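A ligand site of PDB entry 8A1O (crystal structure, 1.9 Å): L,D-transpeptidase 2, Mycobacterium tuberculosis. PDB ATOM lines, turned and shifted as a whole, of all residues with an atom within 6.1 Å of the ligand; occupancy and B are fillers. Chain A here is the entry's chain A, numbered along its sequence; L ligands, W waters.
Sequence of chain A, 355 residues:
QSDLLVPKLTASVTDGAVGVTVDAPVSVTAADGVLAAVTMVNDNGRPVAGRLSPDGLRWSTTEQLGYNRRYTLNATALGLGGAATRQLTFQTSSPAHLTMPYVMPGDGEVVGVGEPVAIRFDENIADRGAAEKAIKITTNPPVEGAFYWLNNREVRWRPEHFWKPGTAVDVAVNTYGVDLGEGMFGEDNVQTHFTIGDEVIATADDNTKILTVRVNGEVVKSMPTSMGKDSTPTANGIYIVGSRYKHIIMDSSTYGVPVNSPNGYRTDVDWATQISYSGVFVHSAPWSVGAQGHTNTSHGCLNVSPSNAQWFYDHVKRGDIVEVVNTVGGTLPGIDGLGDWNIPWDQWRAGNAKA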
ATOM      1  N   LYS A 229     -22.903  -4.309  -0.205  1.00  0.00           N
ATOM      2  CA  LYS A 229     -21.502  -3.975  -0.003  1.00  0.00           C
ATOM      3  C   LYS A 229     -20.948  -3.305  -1.254  1.00  0.00           C
ATOM      4  O   LYS A 229     -21.554  -3.309  -2.330  1.00  0.00           O
ATOM      5  CB  LYS A 229     -20.691  -5.223   0.343  1.00  0.00           C
ATOM      6  CG  LYS A 229     -20.779  -6.324  -0.706  1.00  0.00           C
ATOM      7  CD  LYS A 229     -20.189  -7.620  -0.173  1.00  0.00           C
ATOM      8  CE  LYS A 229     -20.364  -8.763  -1.193  1.00  0.00           C
ATOM      9  NZ  LYS A 229     -21.778  -9.242  -1.263  1.00  0.00           N
ATOM     10  N   MET A 250     -34.888 -19.225  -0.839  1.00  0.00           N
ATOM     11  CA  MET A 250     -34.044 -18.749  -1.932  1.00  0.00           C
ATOM     12  C   MET A 250     -32.788 -19.609  -2.044  1.00  0.00           C
ATOM     13  O   MET A 250     -32.093 -19.835  -1.054  1.00  0.00           O
ATOM     14  CB  MET A 250     -33.663 -17.290  -1.713  1.00  0.00           C
ATOM     15  CG  MET A 250     -34.832 -16.369  -1.496  1.00  0.00           C
ATOM     16  SD  MET A 250     -34.330 -14.666  -1.684  1.00  0.00           S
ATOM     17  CE  MET A 250     -35.673 -13.782  -0.854  1.00  0.00           C
ATOM     18  N   GLY A 264     -22.902 -17.470  -2.933  1.00  0.00           N
ATOM     19  CA  GLY A 264     -23.965 -18.432  -2.848  1.00  0.00           C
ATOM     20  C   GLY A 264     -24.766 -18.323  -1.570  1.00  0.00           C
ATOM     21  O   GLY A 264     -24.310 -17.784  -0.577  1.00  0.00           O
ATOM     22  N   TYR A 265     -25.970 -18.885  -1.595  1.00  0.00           N
ATOM     23  CA  TYR A 265     -26.876 -18.832  -0.458  1.00  0.00           C
ATOM     24  C   TYR A 265     -27.948 -19.892  -0.636  1.00  0.00           C
ATOM     25  O   TYR A 265     -28.291 -20.250  -1.761  1.00  0.00           O
ATOM     26  CB  TYR A 265     -27.527 -17.448  -0.331  1.00  0.00           C
ATOM     27  CG  TYR A 265     -28.153 -16.975  -1.613  1.00  0.00           C
ATOM     28  CD1 TYR A 265     -27.518 -16.047  -2.416  1.00  0.00           C
ATOM     29  CD2 TYR A 265     -29.394 -17.461  -2.028  1.00  0.00           C
ATOM     30  CE1 TYR A 265     -28.111 -15.588  -3.588  1.00  0.00           C
ATOM     31  CE2 TYR A 265     -29.972 -17.040  -3.190  1.00  0.00           C
ATOM     32  CZ  TYR A 265     -29.343 -16.077  -3.962  1.00  0.00           C
ATOM     33  OH  TYR A 265     -29.920 -15.669  -5.144  1.00  0.00           O
ATOM     34  N   ARG A 266     -28.469 -20.373   0.499  1.00  0.00           N
ATOM     35  CA  ARG A 266     -29.591 -21.322   0.487  1.00  0.00           C
ATOM     36  C   ARG A 266     -30.268 -21.203   1.859  1.00  0.00           C
ATOM     37  O   ARG A 266     -29.865 -21.867   2.810  1.00  0.00           O
ATOM     38  CB  ARG A 266     -29.115 -22.730   0.191  1.00  0.00           C
ATOM     39  CG  ARG A 266     -30.232 -23.770   0.033  1.00  0.00           C
ATOM     40  CD  ARG A 266     -29.680 -25.102  -0.404  1.00  0.00           C
ATOM     41  NE  ARG A 266     -28.836 -25.731   0.602  1.00  0.00           N
ATOM     42  CZ  ARG A 266     -28.057 -26.795   0.390  1.00  0.00           C
ATOM     43  NH1 ARG A 266     -27.969 -27.333  -0.831  1.00  0.00           N
ATOM     44  NH2 ARG A 266     -27.336 -27.311   1.394  1.00  0.00           N
ATOM     45  N   THR A 267     -31.323 -20.398   1.925  1.00  0.00           N
ATOM     46  CA  THR A 267     -31.917 -20.084   3.212  1.00  0.00           C
ATOM     47  C   THR A 267     -33.401 -19.780   3.057  1.00  0.00           C
ATOM     48  O   THR A 267     -33.882 -19.402   1.978  1.00  0.00           O
ATOM     49  CB  THR A 267     -31.210 -18.886   3.888  1.00  0.00           C
ATOM     50  OG1 THR A 267     -31.829 -18.607   5.148  1.00  0.00           O
ATOM     51  CG2 THR A 267     -31.324 -17.645   3.034  1.00  0.00           C
ATOM     52  N   VAL A 269     -35.914 -17.135   4.110  1.00  0.00           N
ATOM     53  CA  VAL A 269     -35.820 -15.735   4.540  1.00  0.00           C
ATOM     54  C   VAL A 269     -37.156 -15.293   5.102  1.00  0.00           C
ATOM     55  O   VAL A 269     -38.208 -15.587   4.526  1.00  0.00           O
ATOM     56  CB  VAL A 269     -35.400 -14.833   3.351  1.00  0.00           C
ATOM     57  CG1 VAL A 269     -35.233 -13.396   3.794  1.00  0.00           C
ATOM     58  CG2 VAL A 269     -34.149 -15.365   2.688  1.00  0.00           C
ATOM     59  N   GLY A 279     -33.987  -8.451  -7.861  1.00  0.00           N
ATOM     60  CA  GLY A 279     -33.779  -9.212  -6.649  1.00  0.00           C
ATOM     61  C   GLY A 279     -33.537  -8.418  -5.399  1.00  0.00           C
ATOM     62  O   GLY A 279     -33.010  -8.979  -4.426  1.00  0.00           O
ATOM     63  N   VAL A 280     -33.850  -7.139  -5.378  1.00  0.00           N
ATOM     64  CA  VAL A 280     -33.637  -6.334  -4.184  1.00  0.00           C
ATOM     65  C   VAL A 280     -34.857  -6.526  -3.290  1.00  0.00           C
ATOM     66  O   VAL A 280     -36.002  -6.298  -3.704  1.00  0.00           O
ATOM     67  CB  VAL A 280     -33.417  -4.862  -4.531  1.00  0.00           C
ATOM     68  CG1 VAL A 280     -33.297  -4.054  -3.279  1.00  0.00           C
ATOM     69  CG2 VAL A 280     -32.197  -4.654  -5.382  1.00  0.00           C
ATOM     70  N   PHE A 281     -34.615  -6.948  -2.061  1.00  0.00           N
ATOM     71  CA  PHE A 281     -35.650  -7.156  -1.065  1.00  0.00           C
ATOM     72  C   PHE A 281     -35.329  -6.356   0.189  1.00  0.00           C
ATOM     73  O   PHE A 281     -34.163  -6.112   0.502  1.00  0.00           O
ATOM     74  CB  PHE A 281     -35.778  -8.669  -0.689  1.00  0.00           C
ATOM     75  CG  PHE A 281     -36.406  -9.508  -1.726  1.00  0.00           C
ATOM     76  CD1 PHE A 281     -37.697  -9.996  -1.550  1.00  0.00           C
ATOM     77  CD2 PHE A 281     -35.711  -9.848  -2.878  1.00  0.00           C
ATOM     78  CE1 PHE A 281     -38.278 -10.791  -2.516  1.00  0.00           C
ATOM     79  CE2 PHE A 281     -36.287 -10.642  -3.836  1.00  0.00           C
ATOM     80  CZ  PHE A 281     -37.598 -11.103  -3.677  1.00  0.00           C
ATOM     81  N   HIS A 283     -35.735  -7.333   3.975  1.00  0.00           N
ATOM     82  CA  HIS A 283     -35.989  -8.574   4.696  1.00  0.00           C
ATOM     83  C   HIS A 283     -35.249  -8.616   6.041  1.00  0.00           C
ATOM     84  O   HIS A 283     -34.378  -7.792   6.359  1.00  0.00           O
ATOM     85  CB  HIS A 283     -35.629  -9.805   3.829  1.00  0.00           C
ATOM     86  CG  HIS A 283     -34.163  -9.999   3.612  1.00  0.00           C
ATOM     87  ND1 HIS A 283     -33.319 -10.470   4.592  1.00  0.00           N
ATOM     88  CD2 HIS A 283     -33.395  -9.823   2.507  1.00  0.00           C
ATOM     89  CE1 HIS A 283     -32.090 -10.533   4.121  1.00  0.00           C
ATOM     90  NE2 HIS A 283     -32.106 -10.153   2.854  1.00  0.00           N
ATOM     91  N   SER A 284     -35.602  -9.621   6.829  1.00  0.00           N
ATOM     92  CA  SER A 284     -35.007  -9.799   8.133  1.00  0.00           C
ATOM     93  C   SER A 284     -33.586 -10.347   8.010  1.00  0.00           C
ATOM     94  O   SER A 284     -33.369 -11.356   7.346  1.00  0.00           O
ATOM     95  CB  SER A 284     -35.851 -10.755   8.967  1.00  0.00           C
ATOM     96  OG  SER A 284     -35.212 -11.004  10.181  1.00  0.00           O
ATOM     97  N   ALA A 285     -32.627  -9.704   8.664  1.00  0.00           N
ATOM     98  CA  ALA A 285     -31.230 -10.138   8.647  1.00  0.00           C
ATOM     99  C   ALA A 285     -30.717 -10.132  10.075  1.00  0.00           C
ATOM    100  O   ALA A 285     -29.981  -9.203  10.477  1.00  0.00           O
ATOM    101  CB  ALA A 285     -30.401  -9.243   7.740  1.00  0.00           C
ATOM    102  N   TRP A 287     -28.427 -11.837  11.374  1.00  0.00           N
ATOM    103  CA  TRP A 287     -26.982 -12.023  11.449  1.00  0.00           C
ATOM    104  C   TRP A 287     -26.227 -10.711  11.324  1.00  0.00           C
ATOM    105  O   TRP A 287     -25.079 -10.618  11.784  1.00  0.00           O
ATOM    106  CB  TRP A 287     -26.528 -12.969  10.339  1.00  0.00           C
ATOM    107  CG  TRP A 287     -26.975 -12.504   8.992  1.00  0.00           C
ATOM    108  CD1 TRP A 287     -26.332 -11.630   8.160  1.00  0.00           C
ATOM    109  CD2 TRP A 287     -28.202 -12.874   8.312  1.00  0.00           C
ATOM    110  NE1 TRP A 287     -27.066 -11.440   7.002  1.00  0.00           N
ATOM    111  CE2 TRP A 287     -28.213 -12.187   7.071  1.00  0.00           C
ATOM    112  CE3 TRP A 287     -29.270 -13.724   8.630  1.00  0.00           C
ATOM    113  CZ2 TRP A 287     -29.253 -12.336   6.158  1.00  0.00           C
ATOM    114  CZ3 TRP A 287     -30.301 -13.862   7.711  1.00  0.00           C
ATOM    115  CH2 TRP A 287     -30.282 -13.171   6.487  1.00  0.00           C
ATOM    116  N   SER A 288     -26.847  -9.689  10.716  1.00  0.00           N
ATOM    117  CA  SER A 288     -26.179  -8.420  10.461  1.00  0.00           C
ATOM    118  C   SER A 288     -26.722  -7.282  11.323  1.00  0.00           C
ATOM    119  O   SER A 288     -26.556  -6.108  10.962  1.00  0.00           O
ATOM    120  CB  SER A 288     -26.289  -8.065   8.985  1.00  0.00           C
ATOM    121  OG  SER A 288     -27.651  -7.865   8.606  1.00  0.00           O
ATOM    122  N   THR A 297     -23.308  -4.750   4.022  1.00  0.00           N
ATOM    123  CA  THR A 297     -22.823  -6.125   4.033  1.00  0.00           C
ATOM    124  C   THR A 297     -23.574  -7.057   3.107  1.00  0.00           C
ATOM    125  O   THR A 297     -23.196  -8.233   2.991  1.00  0.00           O
ATOM    126  CB  THR A 297     -22.894  -6.689   5.465  1.00  0.00           C
ATOM    127  OG1 THR A 297     -24.276  -6.692   5.899  1.00  0.00           O
ATOM    128  CG2 THR A 297     -22.064  -5.868   6.437  1.00  0.00           C
ATOM    129  N   SER A 298     -24.627  -6.597   2.426  1.00  0.00           N
ATOM    130  CA  SER A 298     -25.462  -7.528   1.690  1.00  0.00           C
ATOM    131  C   SER A 298     -25.020  -7.633   0.230  1.00  0.00           C
ATOM    132  O   SER A 298     -24.062  -6.989  -0.213  1.00  0.00           O
ATOM    133  CB  SER A 298     -26.918  -7.069   1.767  1.00  0.00           C
ATOM    134  OG  SER A 298     -27.126  -5.990   0.886  1.00  0.00           O
ATOM    135  N   HIS A 299     -25.793  -8.351  -0.608  1.00  0.00           N
ATOM    136  CA  HIS A 299     -25.575  -8.439  -2.071  1.00  0.00           C
ATOM    137  C   HIS A 299     -26.412  -7.390  -2.824  1.00  0.00           C
ATOM    138  O   HIS A 299     -26.366  -7.446  -4.049  1.00  0.00           O
ATOM    139  CB  HIS A 299     -25.968  -9.804  -2.629  1.00  0.00           C
ATOM    140  CG  HIS A 299     -25.237 -10.967  -2.064  1.00  0.00           C
ATOM    141  ND1 HIS A 299     -24.094 -10.836  -1.325  1.00  0.00           N
ATOM    142  CD2 HIS A 299     -25.459 -12.289  -2.171  1.00  0.00           C
ATOM    143  CE1 HIS A 299     -23.660 -12.015  -0.971  1.00  0.00           C
ATOM    144  NE2 HIS A 299     -24.482 -12.924  -1.480  1.00  0.00           N
ATOM    145  N   GLY A 300     -27.096  -6.459  -2.151  1.00  0.00           N
ATOM    146  CA  GLY A 300     -27.979  -5.439  -2.728  1.00  0.00           C
ATOM    147  C   GLY A 300     -29.267  -5.267  -1.952  1.00  0.00           C
ATOM    148  O   GLY A 300     -29.863  -4.203  -2.047  1.00  0.00           O
ATOM    149  N   CYS A 301     -29.665  -6.251  -1.145  1.00  0.00           N
ATOM    150  CA  CYS A 301     -30.851  -6.134  -0.365  1.00  0.00           C
ATOM    151  C   CYS A 301     -30.745  -5.114   0.745  1.00  0.00           C
ATOM    152  O   CYS A 301     -29.707  -4.816   1.203  1.00  0.00           O
ATOM    153  CB  CYS A 301     -31.057  -7.428   0.386  1.00  0.00           C
ATOM    154  SG  CYS A 301     -31.830  -8.678  -0.644  1.00  0.00           S
ATOM    155  N   LEU A 302     -31.891  -4.560   1.080  1.00  0.00           N
ATOM    156  CA  LEU A 302     -31.816  -3.675   2.330  1.00  0.00           C
ATOM    157  C   LEU A 302     -32.044  -4.559   3.567  1.00  0.00           C
ATOM    158  O   LEU A 302     -33.189  -4.881   3.856  1.00  0.00           O
ATOM    159  CB  LEU A 302     -32.923  -2.633   2.224  1.00  0.00           C
ATOM    160  CG  LEU A 302     -32.664  -1.397   1.399  1.00  0.00           C
ATOM    161  CD1 LEU A 302     -32.107  -1.764   0.038  1.00  0.00           C
ATOM    162  CD2 LEU A 302     -33.941  -0.585   1.247  1.00  0.00           C
ATOM    163  N   ASN A 303     -30.989  -4.990   4.230  1.00  0.00           N
ATOM    164  CA  ASN A 303     -31.077  -5.817   5.455  1.00  0.00           C
ATOM    165  C   ASN A 303     -31.584  -4.952   6.593  1.00  0.00           C
ATOM    166  O   ASN A 303     -31.078  -3.880   6.736  1.00  0.00           O
ATOM    167  CB  ASN A 303     -29.686  -6.278   5.830  1.00  0.00           C
ATOM    168  CG  ASN A 303     -29.172  -7.458   5.046  1.00  0.00           C
ATOM    169  OD1 ASN A 303     -28.082  -7.912   5.311  1.00  0.00           O
ATOM    170  ND2 ASN A 303     -29.930  -7.911   4.077  1.00  0.00           N
HETATM  171  C1  LIG L   1     -30.996 -11.033  -1.504  1.00  0.00           C
HETATM  172  C2  LIG L   1     -30.597 -13.950  -1.054  1.00  0.00           C
HETATM  173  C3  LIG L   1     -31.035 -13.452   1.345  1.00  0.00           C
HETATM  174  C4  LIG L   1     -30.683 -13.450   2.673  1.00  0.00           C
HETATM  175  C5  LIG L   1     -28.941 -14.438   0.765  1.00  0.00           C
HETATM  176  C6  LIG L   1     -27.997 -10.768   1.959  1.00  0.00           C
HETATM  177  C7  LIG L   1     -27.005 -10.627   4.005  1.00  0.00           C
HETATM  178  C8  LIG L   1     -29.310  -9.885  -0.077  1.00  0.00           C
HETATM  179  C9  LIG L   1     -30.633  -9.993  -0.798  1.00  0.00           C
HETATM  180  C10 LIG L   1     -30.168 -13.955   0.406  1.00  0.00           C
HETATM  181  C11 LIG L   1     -29.456 -13.943   3.034  1.00  0.00           C
HETATM  182  C12 LIG L   1     -28.589 -14.436   2.094  1.00  0.00           C
HETATM  183  C13 LIG L   1     -25.797 -11.009   3.498  1.00  0.00           C
HETATM  184  C14 LIG L   1     -24.656 -10.160   5.339  1.00  0.00           C
HETATM  185  C15 LIG L   1     -25.696 -11.319   2.164  1.00  0.00           C
HETATM  186  C16 LIG L   1     -26.827 -11.213   1.378  1.00  0.00           C
HETATM  187  N1  LIG L   1     -29.185 -10.672   1.125  1.00  0.00           N
HETATM  188  N2  LIG L   1     -28.050 -10.514   3.233  1.00  0.00           N
HETATM  189  O1  LIG L   1     -28.448  -9.186  -0.446  1.00  0.00           O
HETATM  190  O2  LIG L   1     -28.627 -12.164  -1.643  1.00  0.00           O
HETATM  191  O3  LIG L   1     -30.010 -12.632  -3.257  1.00  0.00           O
HETATM  192  O4  LIG L   1     -24.698 -11.121   4.334  1.00  0.00           O
HETATM  193  S1  LIG L   1     -29.991 -12.458  -1.859  1.00  0.00           S
HETATM  194 CL1  LIG L   1     -32.602 -12.841   0.818  1.00  0.00          CL
HETATM  195 CL2  LIG L   1     -32.560 -11.093  -2.281  1.00  0.00          CL
HETATM  196  O   HOH W   1     -22.738 -10.145   8.051  1.00  0.00           O
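Merely in contact with the ligand: Gly 279 (3.0 Å), Trp 287 (3.1 Å), Thr 297 (3.4 Å), Ser 298 (3.4 Å), Phe 281 (3.4 Å), Val 269 (3.5 Å), Tyr 265 (3.5 Å) and Met 250 (3.5 Å). Hydrophobic or aromatic side chains that line the ligand: Met 250, Tyr 265, Val 269, Phe 281, His 283, Trp 287 and His 299. The nearest printed residue that does not touch the ligand is Thr 267 (4.1 Å).
N of His 299 is in hydrogen-bond range of O1 of the ligand (2.8 Å). A ring nitrogen (NE2) of His 283 lies within hydrogen-bond range of a nitrogen (N1) of the ligand, at 3.4 Å. The backbone NH (N) of Gly 300 sits at hydrogen-bond distance from an oxygen (O1) of the ligand (3.5 Å). N2 of the ligand is in hydrogen-bond range of ND2 of Asn 303, 3.3 Å away. O1 of the ligand is in hydrogen-bond range of N of Cys 301. A carbon (C9) of the ligand is covalently linked to the side-chain sulfur of Cys 301 (1.8 Å).
The backbone carbonyl oxygen (O) of Cys 301 sits at hydrogen-bond distance from the side-chain hydroxyl (OG) of Ser 298, at 2.9 Å. The backbone NH (N) of Met 250 is in hydrogen-bond range of the backbone carbonyl oxygen (O) of Thr 267 (3.0 Å). ND2 of Asn 303 sits at hydrogen-bond distance from NE2 of His 283, at 3.4 Å. OG of Ser 298 is in hydrogen-bond range of N of Gly 300 (3.1 Å). ND1 of His 299 sits at hydrogen-bond distance from NZ of Lys 229 (2.8 Å). The backbone carbonyl oxygen of Phe 281 is in hydrogen-bond range of the backbone NH of Leu 302, 2.8 Å away. OG of Ser 288 lies within hydrogen-bond range of OD1 of Asn 303 (3.3 Å). O of Ser 298 sits at hydrogen-bond distance from N of Lys 229, 2.9 Å away.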
